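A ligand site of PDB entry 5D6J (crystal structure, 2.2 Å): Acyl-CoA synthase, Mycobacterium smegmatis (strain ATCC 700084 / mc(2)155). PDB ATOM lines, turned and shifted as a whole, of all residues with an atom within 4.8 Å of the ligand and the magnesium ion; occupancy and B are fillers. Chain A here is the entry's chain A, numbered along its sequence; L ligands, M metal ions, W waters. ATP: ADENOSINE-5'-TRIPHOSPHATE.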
ATOM      1  N   THR A 187      36.378   0.714  14.751  1.00  0.00           N
ATOM      2  CA  THR A 187      34.948   0.461  14.571  1.00  0.00           C
ATOM      3  C   THR A 187      34.589  -0.915  15.114  1.00  0.00           C
ATOM      4  O   THR A 187      35.481  -1.709  15.407  1.00  0.00           O
ATOM      5  CB  THR A 187      34.547   0.553  13.089  1.00  0.00           C
ATOM      6  OG1 THR A 187      35.218  -0.467  12.346  1.00  0.00           O
ATOM      7  CG2 THR A 187      34.911   1.911  12.509  1.00  0.00           C
ATOM      8  N   SER A 188      33.297  -1.187  15.254  1.00  0.00           N
ATOM      9  CA  SER A 188      32.855  -2.462  15.814  1.00  0.00           C
ATOM     10  C   SER A 188      33.056  -3.631  14.844  1.00  0.00           C
ATOM     11  O   SER A 188      32.980  -4.787  15.232  1.00  0.00           O
ATOM     12  CB  SER A 188      31.382  -2.392  16.210  1.00  0.00           C
ATOM     13  OG  SER A 188      31.206  -1.480  17.284  1.00  0.00           O
ATOM     14  N   GLY A 189      33.309  -3.316  13.576  1.00  0.00           N
ATOM     15  CA  GLY A 189      33.461  -4.350  12.572  1.00  0.00           C
ATOM     16  C   GLY A 189      32.153  -5.033  12.237  1.00  0.00           C
ATOM     17  O   GLY A 189      32.121  -6.253  12.037  1.00  0.00           O
ATOM     18  N   SER A 190      31.069  -4.271  12.182  1.00  0.00           N
ATOM     19  CA  SER A 190      29.755  -4.815  11.866  1.00  0.00           C
ATOM     20  C   SER A 190      29.623  -5.201  10.395  1.00  0.00           C
ATOM     21  O   SER A 190      28.981  -6.185  10.061  1.00  0.00           O
ATOM     22  CB  SER A 190      28.655  -3.818  12.248  1.00  0.00           C
ATOM     23  OG  SER A 190      28.657  -3.567  13.655  1.00  0.00           O
ATOM     24  N   THR A 191      30.238  -4.419   9.508  1.00  0.00           N
ATOM     25  CA  THR A 191      30.076  -4.618   8.076  1.00  0.00           C
ATOM     26  C   THR A 191      31.397  -4.971   7.379  1.00  0.00           C
ATOM     27  O   THR A 191      31.432  -5.082   6.152  1.00  0.00           O
ATOM     28  CB  THR A 191      29.498  -3.358   7.393  1.00  0.00           C
ATOM     29  OG1 THR A 191      30.490  -2.322   7.385  1.00  0.00           O
ATOM     30  CG2 THR A 191      28.254  -2.878   8.130  1.00  0.00           C
ATOM     31  N   ARG A 192      32.462  -5.141   8.155  1.00  0.00           N
ATOM     32  CA  ARG A 192      33.814  -5.279   7.615  1.00  0.00           C
ATOM     33  C   ARG A 192      34.788  -5.627   8.722  1.00  0.00           C
ATOM     34  O   ARG A 192      34.387  -5.783   9.882  1.00  0.00           O
ATOM     35  CB  ARG A 192      34.248  -3.974   6.953  1.00  0.00           C
ATOM     36  CG  ARG A 192      34.135  -2.807   7.936  1.00  0.00           C
ATOM     37  CD  ARG A 192      34.700  -1.502   7.425  1.00  0.00           C
ATOM     38  NE  ARG A 192      34.228  -0.403   8.284  1.00  0.00           N
ATOM     39  CZ  ARG A 192      34.478   0.879   8.056  1.00  0.00           C
ATOM     40  NH1 ARG A 192      35.210   1.238   7.009  1.00  0.00           N
ATOM     41  NH2 ARG A 192      34.010   1.804   8.883  1.00  0.00           N
ATOM     42  N   ILE A 193      36.061  -5.745   8.382  1.00  0.00           N
ATOM     43  CA  ILE A 193      37.136  -5.811   9.378  1.00  0.00           C
ATOM     44  C   ILE A 193      37.162  -4.482  10.131  1.00  0.00           C
ATOM     45  O   ILE A 193      37.045  -3.426   9.509  1.00  0.00           O
ATOM     46  CB  ILE A 193      38.508  -6.083   8.718  1.00  0.00           C
ATOM     47  CG1 ILE A 193      38.493  -7.422   7.981  1.00  0.00           C
ATOM     48  CG2 ILE A 193      39.638  -6.077   9.755  1.00  0.00           C
ATOM     49  CD1 ILE A 193      39.641  -7.584   7.003  1.00  0.00           C
ATOM     50  N   PRO A 194      37.297  -4.530  11.463  1.00  0.00           N
ATOM     51  CA  PRO A 194      37.390  -3.294  12.256  1.00  0.00           C
ATOM     52  C   PRO A 194      38.413  -2.313  11.668  1.00  0.00           C
ATOM     53  O   PRO A 194      39.533  -2.706  11.347  1.00  0.00           O
ATOM     54  CB  PRO A 194      37.816  -3.785  13.635  1.00  0.00           C
ATOM     55  CG  PRO A 194      37.207  -5.166  13.733  1.00  0.00           C
ATOM     56  CD  PRO A 194      37.280  -5.726  12.325  1.00  0.00           C
ATOM     57  N   ASP A 232      33.619   2.090  21.635  1.00  0.00           N
ATOM     58  CA  ASP A 232      33.373   3.507  21.359  1.00  0.00           C
ATOM     59  C   ASP A 232      32.836   4.263  22.580  1.00  0.00           C
ATOM     60  O   ASP A 232      33.430   5.256  23.034  1.00  0.00           O
ATOM     61  CB  ASP A 232      32.394   3.623  20.199  1.00  0.00           C
ATOM     62  CG  ASP A 232      32.538   4.923  19.446  1.00  0.00           C
ATOM     63  OD1 ASP A 232      33.579   5.592  19.597  1.00  0.00           O
ATOM     64  OD2 ASP A 232      31.590   5.281  18.700  1.00  0.00           O
ATOM     65  N   GLY A 313      23.405   3.861  23.159  1.00  0.00           N
ATOM     66  CA  GLY A 313      23.917   3.931  21.812  1.00  0.00           C
ATOM     67  C   GLY A 313      24.397   2.624  21.207  1.00  0.00           C
ATOM     68  O   GLY A 313      24.164   1.542  21.771  1.00  0.00           O
ATOM     69  N   SER A 314      25.076   2.749  20.068  1.00  0.00           N
ATOM     70  CA  SER A 314      25.587   1.662  19.232  1.00  0.00           C
ATOM     71  C   SER A 314      24.481   0.937  18.466  1.00  0.00           C
ATOM     72  O   SER A 314      24.762   0.101  17.617  1.00  0.00           O
ATOM     73  CB  SER A 314      26.388   0.646  20.063  1.00  0.00           C
ATOM     74  OG  SER A 314      25.528  -0.263  20.728  1.00  0.00           O
ATOM     75  N   GLU A 315      23.230   1.302  18.750  1.00  0.00           N
ATOM     76  CA  GLU A 315      22.086   0.543  18.251  1.00  0.00           C
ATOM     77  C   GLU A 315      20.795   1.329  18.483  1.00  0.00           C
ATOM     78  O   GLU A 315      20.767   2.245  19.296  1.00  0.00           O
ATOM     79  CB  GLU A 315      22.014  -0.800  18.963  1.00  0.00           C
ATOM     80  CG  GLU A 315      21.756  -0.671  20.460  1.00  0.00           C
ATOM     81  CD  GLU A 315      21.766  -2.007  21.181  1.00  0.00           C
ATOM     82  OE1 GLU A 315      22.171  -2.036  22.370  1.00  0.00           O
ATOM     83  OE2 GLU A 315      21.365  -3.020  20.582  1.00  0.00           O
ATOM     84  N   PRO A 316      19.716   0.967  17.767  1.00  0.00           N
ATOM     85  CA  PRO A 316      18.425   1.588  18.082  1.00  0.00           C
ATOM     86  C   PRO A 316      17.882   1.095  19.419  1.00  0.00           C
ATOM     87  O   PRO A 316      17.932  -0.105  19.699  1.00  0.00           O
ATOM     88  CB  PRO A 316      17.520   1.133  16.923  1.00  0.00           C
ATOM     89  CG  PRO A 316      18.115  -0.177  16.485  1.00  0.00           C
ATOM     90  CD  PRO A 316      19.603  -0.007  16.663  1.00  0.00           C
ATOM     91  N   SER A 342      20.712   7.720  21.555  1.00  0.00           N
ATOM     92  CA  SER A 342      21.663   8.581  20.862  1.00  0.00           C
ATOM     93  C   SER A 342      22.181   7.933  19.597  1.00  0.00           C
ATOM     94  O   SER A 342      22.141   6.720  19.441  1.00  0.00           O
ATOM     95  CB  SER A 342      22.843   8.920  21.772  1.00  0.00           C
ATOM     96  OG  SER A 342      23.696   7.800  21.909  1.00  0.00           O
ATOM     97  N   TYR A 343      22.696   8.774  18.697  1.00  0.00           N
ATOM     98  CA  TYR A 343      23.388   8.315  17.515  1.00  0.00           C
ATOM     99  C   TYR A 343      24.878   8.598  17.703  1.00  0.00           C
ATOM    100  O   TYR A 343      25.268   9.692  18.106  1.00  0.00           O
ATOM    101  CB  TYR A 343      22.852   8.989  16.260  1.00  0.00           C
ATOM    102  CG  TYR A 343      23.516   8.589  14.959  1.00  0.00           C
ATOM    103  CD1 TYR A 343      23.640   7.241  14.607  1.00  0.00           C
ATOM    104  CD2 TYR A 343      23.997   9.547  14.072  1.00  0.00           C
ATOM    105  CE1 TYR A 343      24.240   6.868  13.405  1.00  0.00           C
ATOM    106  CE2 TYR A 343      24.600   9.186  12.862  1.00  0.00           C
ATOM    107  CZ  TYR A 343      24.709   7.840  12.534  1.00  0.00           C
ATOM    108  OH  TYR A 343      25.311   7.478  11.348  1.00  0.00           O
ATOM    109  N   GLY A 344      25.700   7.597  17.407  1.00  0.00           N
ATOM    110  CA  GLY A 344      27.129   7.727  17.510  1.00  0.00           C
ATOM    111  C   GLY A 344      27.867   6.709  16.648  1.00  0.00           C
ATOM    112  O   GLY A 344      27.286   5.717  16.228  1.00  0.00           O
ATOM    113  N   LEU A 345      29.141   6.978  16.405  1.00  0.00           N
ATOM    114  CA  LEU A 345      29.987   6.096  15.609  1.00  0.00           C
ATOM    115  C   LEU A 345      31.441   6.529  15.753  1.00  0.00           C
ATOM    116  O   LEU A 345      31.715   7.675  16.125  1.00  0.00           O
ATOM    117  CB  LEU A 345      29.571   6.084  14.124  1.00  0.00           C
ATOM    118  CG  LEU A 345      29.700   7.338  13.259  1.00  0.00           C
ATOM    119  CD1 LEU A 345      29.482   6.983  11.779  1.00  0.00           C
ATOM    120  CD2 LEU A 345      28.727   8.425  13.674  1.00  0.00           C
ATOM    121  N   ALA A 346      32.352   5.611  15.475  1.00  0.00           N
ATOM    122  CA  ALA A 346      33.778   5.876  15.659  1.00  0.00           C
ATOM    123  C   ALA A 346      34.242   7.076  14.845  1.00  0.00           C
ATOM    124  O   ALA A 346      35.097   7.846  15.302  1.00  0.00           O
ATOM    125  CB  ALA A 346      34.602   4.632  15.280  1.00  0.00           C
ATOM    126  N   GLU A 347      33.691   7.237  13.637  1.00  0.00           N
ATOM    127  CA  GLU A 347      34.115   8.301  12.724  1.00  0.00           C
ATOM    128  C   GLU A 347      33.882   9.702  13.320  1.00  0.00           C
ATOM    129  O   GLU A 347      34.545  10.675  12.952  1.00  0.00           O
ATOM    130  CB  GLU A 347      33.400   8.195  11.375  1.00  0.00           C
ATOM    131  CG  GLU A 347      33.873   7.062  10.454  1.00  0.00           C
ATOM    132  CD  GLU A 347      33.272   5.701  10.791  1.00  0.00           C
ATOM    133  OE1 GLU A 347      32.581   5.565  11.831  1.00  0.00           O
ATOM    134  OE2 GLU A 347      33.468   4.761   9.996  1.00  0.00           O
ATOM    135  N   ALA A 392      16.870   9.110  17.433  1.00  0.00           N
ATOM    136  CA  ALA A 392      18.185   9.393  17.991  1.00  0.00           C
ATOM    137  C   ALA A 392      18.299  10.865  18.400  1.00  0.00           C
ATOM    138  O   ALA A 392      19.384  11.353  18.723  1.00  0.00           O
ATOM    139  CB  ALA A 392      19.281   9.018  17.002  1.00  0.00           C
ATOM    140  N   THR A 467      28.652   7.938   6.687  1.00  0.00           N
ATOM    141  CA  THR A 467      28.522   7.076   7.850  1.00  0.00           C
ATOM    142  C   THR A 467      28.357   5.593   7.503  1.00  0.00           C
ATOM    143  O   THR A 467      28.709   4.728   8.306  1.00  0.00           O
ATOM    144  CB  THR A 467      27.326   7.490   8.719  1.00  0.00           C
ATOM    145  OG1 THR A 467      26.116   7.358   7.954  1.00  0.00           O
ATOM    146  CG2 THR A 467      27.490   8.945   9.205  1.00  0.00           C
ATOM    147  N   ASP A 469      25.340   4.550   6.961  1.00  0.00           N
ATOM    148  CA  ASP A 469      23.976   4.322   7.453  1.00  0.00           C
ATOM    149  C   ASP A 469      22.920   4.973   6.580  1.00  0.00           C
ATOM    150  O   ASP A 469      23.147   6.033   6.007  1.00  0.00           O
ATOM    151  CB  ASP A 469      23.823   4.862   8.873  1.00  0.00           C
ATOM    152  CG  ASP A 469      24.772   4.219   9.863  1.00  0.00           C
ATOM    153  OD1 ASP A 469      25.024   3.001   9.733  1.00  0.00           O
ATOM    154  OD2 ASP A 469      25.264   4.932  10.764  1.00  0.00           O
ATOM    155  N   ILE A 480      17.724   6.310  12.329  1.00  0.00           N
ATOM    156  CA  ILE A 480      18.620   5.474  11.533  1.00  0.00           C
ATOM    157  C   ILE A 480      17.838   4.220  11.140  1.00  0.00           C
ATOM    158  O   ILE A 480      17.438   3.438  12.011  1.00  0.00           O
ATOM    159  CB  ILE A 480      19.917   5.078  12.294  1.00  0.00           C
ATOM    160  CG1 ILE A 480      20.871   6.269  12.441  1.00  0.00           C
ATOM    161  CG2 ILE A 480      20.636   3.966  11.543  1.00  0.00           C
ATOM    162  CD1 ILE A 480      20.445   7.326  13.453  1.00  0.00           C
ATOM    163  N   ARG A 483      21.771  -0.148   7.843  1.00  0.00           N
ATOM    164  CA  ARG A 483      23.108  -0.006   7.279  1.00  0.00           C
ATOM    165  C   ARG A 483      23.080  -0.162   5.765  1.00  0.00           C
ATOM    166  O   ARG A 483      22.455  -1.091   5.249  1.00  0.00           O
ATOM    167  CB  ARG A 483      24.059  -1.027   7.902  1.00  0.00           C
ATOM    168  CG  ARG A 483      24.138  -0.970   9.437  1.00  0.00           C
ATOM    169  CD  ARG A 483      25.064  -2.071   9.972  1.00  0.00           C
ATOM    170  NE  ARG A 483      25.241  -1.997  11.423  1.00  0.00           N
ATOM    171  CZ  ARG A 483      26.173  -1.265  12.028  1.00  0.00           C
ATOM    172  NH1 ARG A 483      27.020  -0.542  11.305  1.00  0.00           N
ATOM    173  NH2 ARG A 483      26.258  -1.257  13.354  1.00  0.00           N
HETATM  174  PG  ATP L   1      31.843  -0.814  10.920  1.00  0.00           P
HETATM  175  O1G ATP L   1      32.008   0.685  10.801  1.00  0.00           O
HETATM  176  O2G ATP L   1      30.855  -1.446   9.971  1.00  0.00           O
HETATM  177  O3G ATP L   1      33.182  -1.510  10.959  1.00  0.00           O
HETATM  178  PB  ATP L   1      30.145  -0.096  13.131  1.00  0.00           P
HETATM  179  O1B ATP L   1      29.176  -0.926  13.926  1.00  0.00           O
HETATM  180  O2B ATP L   1      29.641   0.925  12.150  1.00  0.00           O
HETATM  181  O3B ATP L   1      31.180  -1.081  12.377  1.00  0.00           O
HETATM  182  PA  ATP L   1      30.798   1.653  15.353  1.00  0.00           P
HETATM  183  O1A ATP L   1      31.249   1.079  16.674  1.00  0.00           O
HETATM  184  O2A ATP L   1      31.341   2.992  14.906  1.00  0.00           O
HETATM  185  O3A ATP L   1      31.173   0.593  14.182  1.00  0.00           O
HETATM  186  O5' ATP L   1      29.197   1.694  15.377  1.00  0.00           O
HETATM  187  C5' ATP L   1      28.447   2.853  15.022  1.00  0.00           C
HETATM  188  C4' ATP L   1      27.204   2.375  14.293  1.00  0.00           C
HETATM  189  O4' ATP L   1      26.230   1.866  15.216  1.00  0.00           O
HETATM  190  C3' ATP L   1      26.449   3.465  13.540  1.00  0.00           C
HETATM  191  O3' ATP L   1      27.026   3.774  12.259  1.00  0.00           O
HETATM  192  C2' ATP L   1      25.077   2.853  13.407  1.00  0.00           C
HETATM  193  O2' ATP L   1      25.086   1.922  12.331  1.00  0.00           O
HETATM  194  C1' ATP L   1      24.909   2.063  14.696  1.00  0.00           C
HETATM  195  N9  ATP L   1      24.129   2.936  15.585  1.00  0.00           N
HETATM  196  C8  ATP L   1      24.621   3.767  16.529  1.00  0.00           C
HETATM  197  N7  ATP L   1      23.616   4.442  17.144  1.00  0.00           N
HETATM  198  C5  ATP L   1      22.457   4.060  16.582  1.00  0.00           C
HETATM  199  C6  ATP L   1      21.019   4.393  16.744  1.00  0.00           C
HETATM  200  N6  ATP L   1      20.613   5.296  17.673  1.00  0.00           N
HETATM  201  N1  ATP L   1      20.141   3.761  15.948  1.00  0.00           N
HETATM  202  C2  ATP L   1      20.528   2.868  15.014  1.00  0.00           C
HETATM  203  N3  ATP L   1      21.801   2.518  14.801  1.00  0.00           N
HETATM  204  C4  ATP L   1      22.800   3.070  15.550  1.00  0.00           C
HETATM  205 MG    MG M   1      30.507   2.022  10.704  1.00  0.00          MG
HETATM  206  O   HOH W   1      29.518   1.304  18.825  1.00  0.00           O
HETATM  207  O   HOH W   2      19.901   4.499  20.811  1.00  0.00           O
HETATM  208  O   HOH W   3      33.722   1.589  17.943  1.00  0.00           O
HETATM  209  O   HOH W   4      17.545   4.737  15.039  1.00  0.00           O
HETATM  210  O   HOH W   5      31.340   3.241   9.302  1.00  0.00           O
HETATM  211  O   HOH W   6      17.847   5.499  19.001  1.00  0.00           O
HETATM  212  O   HOH W   7      28.836   3.211  10.544  1.00  0.00           O
HETATM  213  O   HOH W   8      22.573   0.527  12.852  1.00  0.00           O
HETATM  214  O   HOH W   9      27.336  -0.784  16.433  1.00  0.00           O
HETATM  215  O   HOH W  10      25.582   5.221  19.418  1.00  0.00           O
HETATM  216  O   HOH W  11      29.639   0.793   9.047  1.00  0.00           O
HETATM  217  O   HOH W  12      31.536   3.285  12.162  1.00  0.00           O
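Merely in contact with the magnesium ion: Arg 192 (3.95 Å).
Of the 24 residues printed, 1 comes within 4 Å of the magnesium ion.
The nearest printed residue that does not touch the magnesium ion is Thr 467 (4.04 Å).
O of Ser 314 lies close to O4' of the ligand (3.3 Å).
The backbone nitrogen of Pro 316 lies close to a nitrogen (N1) of the ligand (3.4 Å).
Tyr 343 touches the ligand (CD1 to N7, 3.8 Å).
O of Gly 344 touches C8 of the ligand (3.3 Å).
Leu 345 touches the ligand.
Ile 480 touches the ligand.
Hydrophobic or aromatic side chains that line the ligand: Pro 316, Tyr 343, Leu 345, Ala 346 and Ile 480.
17 residues have an atom within 4 Å of the ligand: Thr 187, Ser 188, Gly 189, Ser 190, Thr 191, Arg 192, Ser 314, Glu 315, Pro 316, Ser 342, Tyr 343, Gly 344, Leu 345, Ala 346, Asp 469, Ile 480 and Arg 483.
The nearest printed residue that does not touch the ligand is Ala 392 (4.01 Å).
Water W12 lies within hydrogen-bond range of the side-chain carboxylate (OE1) of Glu 347 (2.5 Å) and an oxygen (O2A) of the ligand (2.8 Å).
Water W7 lies within hydrogen-bond range of an oxygen (O3') of the ligand (2.6 Å) and the backbone carbonyl oxygen of Thr 467 (2.7 Å).
Water W5 lies within hydrogen-bond range of OE2 of Glu 347 (2.7 Å), NH2 of Arg 192 (3.1 Å) and O of Thr 467 (3.2 Å).
Water W4 bridges N1 of the ligand (2.9 Å) and N of Ile 480 (3.1 Å).
Water W10 lies within hydrogen-bond range of N of Ser 314 (2.6 Å), N7 of the ligand (3.1 Å) and N of Gly 344 (3.1 Å).
Water W2 lies within hydrogen-bond range of the backbone carbonyl oxygen of Glu 315, a nitrogen (N6) of the ligand and the backbone NH of Ser 342.
The magnesium ion is bound by O2B of the ligand, O1G of the ligand, water W5, water W7, water W12 and water W11.
The side-chain carboxylate (OD2) of Asp 469 is in hydrogen-bond range of the side-chain hydroxyl (OH) of Tyr 343 (2.6 Å).
The side-chain hydroxyl of Thr 467 sits at hydrogen-bond distance from the backbone NH of Asp 469, 3.1 Å away.
The side-chain hydroxyl of Ser 190 lies within hydrogen-bond range of the guanidinium group of Arg 483.
The backbone NH (N) of Ala 346 lies within hydrogen-bond range of the side-chain carboxylate (OD2) of Asp 232 (3.3 Å).
The guanidinium group of Arg 192 is in salt-bridge range of the side-chain carboxylate of Glu 347, 3.2 Å away.
OG1 of Thr 467 sits close to OH of Tyr 343 (3.5 Å).
The side-chain carboxylate (OD2) of Asp 469 lies within hydrogen-bond range of an oxygen (O3') of the ligand, at 2.6 Å.
An oxygen (O3A) of the ligand is in hydrogen-bond range of the backbone NH (N) of Ser 188 (3.0 Å).
OG of Ser 188 is in hydrogen-bond range of O1A of the ligand (2.6 Å).
OG1 of Thr 187 lies within hydrogen-bond range of O3G of the ligand, 2.7 Å away.
The backbone NH (N) of Ser 190 sits at hydrogen-bond distance from an oxygen (O3B) of the ligand.
An oxygen (O1B) of the ligand sits at hydrogen-bond distance from the side-chain hydroxyl of Ser 190 (2.7 Å).
The backbone carbonyl oxygen of Ser 342 sits at hydrogen-bond distance from a nitrogen (N6) of the ligand.
An oxygen (O2G) of the ligand lies within hydrogen-bond range of the backbone NH (N) of Thr 191.
O2G of the ligand sits at hydrogen-bond distance from OG1 of Thr 191 (2.8 Å).
An oxygen (O2A) of the ligand sits at hydrogen-bond distance from the backbone NH (N) of Ala 346, 2.9 Å away.
O3G of the ligand lies within salt-bridge range of NE of Arg 192 (3.1 Å).
An oxygen (O1B) of the ligand lies within salt-bridge range of the guanidinium group (NH2) of Arg 483 (3.0 Å).
An oxygen (O3G) of the ligand lies within hydrogen-bond range of the backbone NH (N) of Gly 189.
The backbone carbonyl oxygen (O) of Glu 315 lies close to a nitrogen (N6) of the ligand (3.5 Å).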
